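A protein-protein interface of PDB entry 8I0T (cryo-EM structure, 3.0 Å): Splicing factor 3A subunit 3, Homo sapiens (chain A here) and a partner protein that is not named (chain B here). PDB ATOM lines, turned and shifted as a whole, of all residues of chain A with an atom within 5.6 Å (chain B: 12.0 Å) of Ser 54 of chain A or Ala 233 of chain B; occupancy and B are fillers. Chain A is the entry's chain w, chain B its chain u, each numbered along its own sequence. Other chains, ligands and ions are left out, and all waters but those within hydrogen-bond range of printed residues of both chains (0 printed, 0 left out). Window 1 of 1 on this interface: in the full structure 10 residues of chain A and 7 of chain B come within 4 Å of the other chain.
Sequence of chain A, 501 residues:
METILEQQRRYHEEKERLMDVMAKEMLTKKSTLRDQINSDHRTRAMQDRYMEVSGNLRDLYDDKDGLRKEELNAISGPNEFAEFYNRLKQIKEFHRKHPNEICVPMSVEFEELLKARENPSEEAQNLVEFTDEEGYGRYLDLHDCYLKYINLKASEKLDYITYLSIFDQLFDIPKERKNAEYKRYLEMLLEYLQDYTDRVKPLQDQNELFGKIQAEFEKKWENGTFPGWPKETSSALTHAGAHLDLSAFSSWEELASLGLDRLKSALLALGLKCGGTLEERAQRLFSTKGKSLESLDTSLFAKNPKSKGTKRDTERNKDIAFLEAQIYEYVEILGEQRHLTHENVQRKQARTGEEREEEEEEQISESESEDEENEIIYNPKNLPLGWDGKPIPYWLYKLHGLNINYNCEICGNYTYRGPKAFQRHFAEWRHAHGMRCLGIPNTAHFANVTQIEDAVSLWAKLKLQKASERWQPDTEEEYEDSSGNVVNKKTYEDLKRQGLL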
ATOM      1  N   ARG A  49     -28.226 -21.357 -21.358  1.00  0.00           N
ATOM      2  CA  ARG A  49     -28.666 -20.464 -20.288  1.00  0.00           C
ATOM      3  C   ARG A  49     -28.084 -20.913 -18.953  1.00  0.00           C
ATOM      4  O   ARG A  49     -27.502 -20.110 -18.204  1.00  0.00           O
ATOM      5  N   TYR A  50     -28.217 -22.209 -18.653  1.00  0.00           N
ATOM      6  CA  TYR A  50     -27.423 -22.797 -17.578  1.00  0.00           C
ATOM      7  C   TYR A  50     -25.934 -22.526 -17.785  1.00  0.00           C
ATOM      8  O   TYR A  50     -25.170 -22.460 -16.821  1.00  0.00           O
ATOM      9  N   MET A  51     -25.514 -22.330 -19.038  1.00  0.00           N
ATOM     10  CA  MET A  51     -24.108 -22.097 -19.345  1.00  0.00           C
ATOM     11  C   MET A  51     -23.666 -20.691 -18.963  1.00  0.00           C
ATOM     12  O   MET A  51     -22.542 -20.491 -18.501  1.00  0.00           O
ATOM     13  N   GLU A  52     -24.526 -19.702 -19.168  1.00  0.00           N
ATOM     14  CA  GLU A  52     -24.224 -18.367 -18.661  1.00  0.00           C
ATOM     15  C   GLU A  52     -24.235 -18.358 -17.135  1.00  0.00           C
ATOM     16  O   GLU A  52     -23.350 -17.765 -16.498  1.00  0.00           O
ATOM     17  N   VAL A  53     -25.228 -19.025 -16.534  1.00  0.00           N
ATOM     18  CA  VAL A  53     -25.248 -19.168 -15.078  1.00  0.00           C
ATOM     19  C   VAL A  53     -23.943 -19.782 -14.580  1.00  0.00           C
ATOM     20  O   VAL A  53     -23.355 -19.321 -13.592  1.00  0.00           O
ATOM     21  N   SER A  54     -23.454 -20.817 -15.269  1.00  0.00           N
ATOM     22  CA  SER A  54     -22.245 -21.507 -14.836  1.00  0.00           C
ATOM     23  C   SER A  54     -20.990 -20.690 -15.102  1.00  0.00           C
ATOM     24  O   SER A  54     -20.047 -20.746 -14.312  1.00  0.00           O
ATOM     25  N   GLY A  55     -20.948 -19.938 -16.202  1.00  0.00           N
ATOM     26  CA  GLY A  55     -19.824 -19.049 -16.438  1.00  0.00           C
ATOM     27  C   GLY A  55     -19.753 -17.931 -15.420  1.00  0.00           C
ATOM     28  O   GLY A  55     -18.683 -17.355 -15.196  1.00  0.00           O
ATOM     29  N   ASN A  56     -20.891 -17.599 -14.802  1.00  0.00           N
ATOM     30  CA  ASN A  56     -20.869 -16.657 -13.688  1.00  0.00           C
ATOM     31  C   ASN A  56     -20.494 -17.334 -12.372  1.00  0.00           C
ATOM     32  O   ASN A  56     -19.815 -16.726 -11.536  1.00  0.00           O
ATOM     33  N   LEU A  57     -20.923 -18.579 -12.168  1.00  0.00           N
ATOM     34  CA  LEU A  57     -20.783 -19.229 -10.867  1.00  0.00           C
ATOM     35  C   LEU A  57     -19.493 -20.032 -10.692  1.00  0.00           C
ATOM     36  O   LEU A  57     -19.091 -20.303  -9.554  1.00  0.00           O
ATOM     37  N   ARG A  58     -18.838 -20.441 -11.779  1.00  0.00           N
ATOM     38  CA  ARG A  58     -17.705 -21.351 -11.680  1.00  0.00           C
ATOM     39  C   ARG A  58     -16.379 -20.641 -11.460  1.00  0.00           C
ATOM     40  O   ARG A  58     -15.453 -21.249 -10.914  1.00  0.00           O
ATOM     41  N   ASP A  59     -16.270 -19.381 -11.870  1.00  0.00           N
ATOM     42  CA  ASP A  59     -15.137 -18.534 -11.534  1.00  0.00           C
ATOM     43  C   ASP A  59     -15.487 -17.511 -10.467  1.00  0.00           C
ATOM     44  O   ASP A  59     -14.640 -16.683 -10.120  1.00  0.00           O
ATOM     45  N   PRO B 221     -19.877 -26.611  -0.749  1.00  0.00           N
ATOM     46  CA  PRO B 221     -18.680 -26.179  -1.486  1.00  0.00           C
ATOM     47  C   PRO B 221     -18.837 -26.310  -2.994  1.00  0.00           C
ATOM     48  O   PRO B 221     -18.413 -25.406  -3.729  1.00  0.00           O
ATOM     49  CB  PRO B 221     -17.586 -27.109  -0.942  1.00  0.00           C
ATOM     50  CG  PRO B 221     -18.073 -27.489   0.477  1.00  0.00           C
ATOM     51  CD  PRO B 221     -19.523 -27.035   0.617  1.00  0.00           C
ATOM     52  N   PRO B 222     -19.437 -27.384  -3.522  1.00  0.00           N
ATOM     53  CA  PRO B 222     -19.715 -27.402  -4.965  1.00  0.00           C
ATOM     54  C   PRO B 222     -20.836 -26.464  -5.390  1.00  0.00           C
ATOM     55  O   PRO B 222     -21.195 -26.452  -6.573  1.00  0.00           O
ATOM     56  CB  PRO B 222     -20.096 -28.872  -5.238  1.00  0.00           C
ATOM     57  CG  PRO B 222     -19.610 -29.633  -4.073  1.00  0.00           C
ATOM     58  CD  PRO B 222     -19.731 -28.699  -2.920  1.00  0.00           C
ATOM     59  N   LYS B 223     -21.398 -25.688  -4.459  1.00  0.00           N
ATOM     60  CA  LYS B 223     -22.539 -24.829  -4.748  1.00  0.00           C
ATOM     61  C   LYS B 223     -22.186 -23.349  -4.768  1.00  0.00           C
ATOM     62  O   LYS B 223     -23.099 -22.519  -4.829  1.00  0.00           O
ATOM     63  N   GLY B 224     -20.906 -22.990  -4.711  1.00  0.00           N
ATOM     64  CA  GLY B 224     -20.560 -21.586  -4.788  1.00  0.00           C
ATOM     65  C   GLY B 224     -19.764 -21.033  -3.627  1.00  0.00           C
ATOM     66  O   GLY B 224     -19.866 -19.839  -3.325  1.00  0.00           O
ATOM     67  N   LEU B 225     -18.992 -21.878  -2.945  1.00  0.00           N
ATOM     68  CA  LEU B 225     -18.124 -21.385  -1.879  1.00  0.00           C
ATOM     69  C   LEU B 225     -16.716 -21.077  -2.386  1.00  0.00           C
ATOM     70  O   LEU B 225     -16.275 -19.924  -2.347  1.00  0.00           O
ATOM     71  N   PHE B 226     -16.012 -22.092  -2.888  1.00  0.00           N
ATOM     72  CA  PHE B 226     -14.644 -21.905  -3.356  1.00  0.00           C
ATOM     73  C   PHE B 226     -14.318 -22.740  -4.589  1.00  0.00           C
ATOM     74  O   PHE B 226     -13.220 -22.596  -5.145  1.00  0.00           O
ATOM     75  N   SER B 227     -15.235 -23.599  -5.031  1.00  0.00           N
ATOM     76  CA  SER B 227     -15.057 -24.398  -6.230  1.00  0.00           C
ATOM     77  C   SER B 227     -16.293 -24.245  -7.103  1.00  0.00           C
ATOM     78  O   SER B 227     -17.425 -24.211  -6.615  1.00  0.00           O
ATOM     79  N   LYS B 228     -16.061 -24.142  -8.408  1.00  0.00           N
ATOM     80  CA  LYS B 228     -17.124 -23.989  -9.393  1.00  0.00           C
ATOM     81  C   LYS B 228     -16.770 -24.810 -10.624  1.00  0.00           C
ATOM     82  O   LYS B 228     -15.727 -24.585 -11.246  1.00  0.00           O
ATOM     83  N   LEU B 229     -17.638 -25.757 -10.968  1.00  0.00           N
ATOM     84  CA  LEU B 229     -17.407 -26.684 -12.069  1.00  0.00           C
ATOM     85  C   LEU B 229     -18.032 -26.125 -13.337  1.00  0.00           C
ATOM     86  O   LEU B 229     -19.127 -25.554 -13.297  1.00  0.00           O
ATOM     87  N   LYS B 230     -17.345 -26.297 -14.460  1.00  0.00           N
ATOM     88  CA  LYS B 230     -17.774 -25.707 -15.715  1.00  0.00           C
ATOM     89  C   LYS B 230     -18.506 -26.672 -16.630  1.00  0.00           C
ATOM     90  O   LYS B 230     -18.811 -26.300 -17.768  1.00  0.00           O
ATOM     91  N   LYS B 231     -18.796 -27.893 -16.175  1.00  0.00           N
ATOM     92  CA  LYS B 231     -19.635 -28.808 -16.940  1.00  0.00           C
ATOM     93  C   LYS B 231     -21.060 -28.297 -17.090  1.00  0.00           C
ATOM     94  O   LYS B 231     -21.830 -28.882 -17.857  1.00  0.00           O
ATOM     95  N   GLU B 232     -21.429 -27.240 -16.366  1.00  0.00           N
ATOM     96  CA  GLU B 232     -22.692 -26.544 -16.552  1.00  0.00           C
ATOM     97  C   GLU B 232     -22.540 -25.275 -17.375  1.00  0.00           C
ATOM     98  O   GLU B 232     -23.345 -25.024 -18.274  1.00  0.00           O
ATOM     99  N   ALA B 233     -21.509 -24.480 -17.096  1.00  0.00           N
ATOM    100  CA  ALA B 233     -21.260 -23.244 -17.821  1.00  0.00           C
ATOM    101  C   ALA B 233     -20.808 -23.461 -19.260  1.00  0.00           C
ATOM    102  O   ALA B 233     -20.903 -22.527 -20.064  1.00  0.00           O
ATOM    103  N   GLU B 234     -20.308 -24.653 -19.602  1.00  0.00           N
ATOM    104  CA  GLU B 234     -19.927 -24.974 -20.972  1.00  0.00           C
ATOM    105  C   GLU B 234     -20.254 -26.420 -21.328  1.00  0.00           C
ATOM    106  O   GLU B 234     -19.512 -27.058 -22.084  1.00  0.00           O
ATOM    107  N   ASN B 235     -21.342 -26.965 -20.780  1.00  0.00           N
ATOM    108  CA  ASN B 235     -21.662 -28.388 -20.903  1.00  0.00           C
ATOM    109  C   ASN B 235     -23.093 -28.617 -21.374  1.00  0.00           C
ATOM    110  O   ASN B 235     -24.023 -28.701 -20.555  1.00  0.00           O
ATOM    111  N   PRO B 236     -23.321 -28.721 -22.686  1.00  0.00           N
ATOM    112  CA  PRO B 236     -24.635 -29.177 -23.157  1.00  0.00           C
ATOM    113  C   PRO B 236     -24.749 -30.688 -23.230  1.00  0.00           C
ATOM    114  O   PRO B 236     -25.867 -31.206 -23.340  1.00  0.00           O
ATOM    115  CB  PRO B 236     -24.758 -28.528 -24.547  1.00  0.00           C
ATOM    116  CG  PRO B 236     -23.543 -27.601 -24.678  1.00  0.00           C
ATOM    117  CD  PRO B 236     -22.506 -28.191 -23.788  1.00  0.00           C
ATOM    118  N   ARG B 237     -23.627 -31.414 -23.162  1.00  0.00           N
ATOM    119  CA  ARG B 237     -23.677 -32.875 -23.164  1.00  0.00           C
ATOM    120  C   ARG B 237     -24.068 -33.412 -21.791  1.00  0.00           C
ATOM    121  O   ARG B 237     -24.942 -34.280 -21.675  1.00  0.00           O
ATOM    122  N   GLU B 238     -23.423 -32.912 -20.734  1.00  0.00           N
ATOM    123  CA  GLU B 238     -23.898 -33.206 -19.388  1.00  0.00           C
ATOM    124  C   GLU B 238     -25.315 -32.686 -19.185  1.00  0.00           C
ATOM    125  O   GLU B 238     -26.079 -33.255 -18.399  1.00  0.00           O
ATOM    126  N   VAL B 239     -25.695 -31.632 -19.912  1.00  0.00           N
ATOM    127  CA  VAL B 239     -27.059 -31.117 -19.831  1.00  0.00           C
ATOM    128  C   VAL B 239     -28.033 -32.088 -20.485  1.00  0.00           C
ATOM    129  O   VAL B 239     -29.153 -32.287 -20.003  1.00  0.00           O
ATOM    130  N   LEU B 240     -27.624 -32.708 -21.596  1.00  0.00           N
ATOM    131  CA  LEU B 240     -28.454 -33.741 -22.209  1.00  0.00           C
ATOM    132  C   LEU B 240     -28.574 -34.954 -21.295  1.00  0.00           C
ATOM    133  O   LEU B 240     -29.657 -35.533 -21.153  1.00  0.00           O
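O of Met 51 of chain A sits close to O of Ala 233 of chain B (3.0 Å).
O of Tyr 50 of chain A lies close to O of Glu 232 of chain B.
The backbone carbonyl oxygen (O) of Arg 58 of chain A sits close to the backbone carbonyl oxygen (O) of Lys 228 of chain B, 3.4 Å away.
Among the printed residues, merely in contact across the chains: Met 51 of chain A with Glu 232 of chain B, Ser 54 of chain A with Ala 233 of chain B and Gly 55 of chain A with Ala 233 of chain B.
Ser 54 of chain A touches one residue of chain B.
Printed residues of chain A within 4 Å of Ala 233 of chain B: Met 51, Ser 54 and Gly 55.
Of chain B, only Glu 232 (3.2 Å) and Ala 233 (3.0 Å) come within 4 Å of Met 51 of chain A.
No residue of chain B comes within 4 Å of Val 53 of chain A.
Gly 55 of chain A touches just one residue of chain B: Ala 233.
No residue of chain B comes within 4 Å of Asn 56 of chain A.
Arg 58 of chain A touches just one residue of chain B: Lys 228.
Printed residues of chain A within 4 Å of Glu 232 of chain B: Tyr 50 (3.5 Å) and Met 51 (3.2 Å).
Of the printed residues of chain A, Lys 228 of chain B touches Arg 58 (3.4 Å).
Pro 222 of chain B touches none of the printed residues of chain A.
Pro 221 of chain B touches none of the printed residues of chain A.
The nearest residue of chain B that does not touch Ser 54 of chain A is Glu 232 of chain B (4.6 Å).
The nearest residue of chain A that does not touch Ala 233 of chain B is Tyr 50 of chain A (4.1 Å).
Printed residues of chain B that touch a printed residue of chain A: Lys 228, Glu 232 and Ala 233.
Of the 11 printed residues of chain A, 5 touch a printed residue of chain B.
Among the printed residues, no Asp or Glu carboxylate lies within 4 Å of a Lys or Arg side-chain nitrogen of the other chain.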
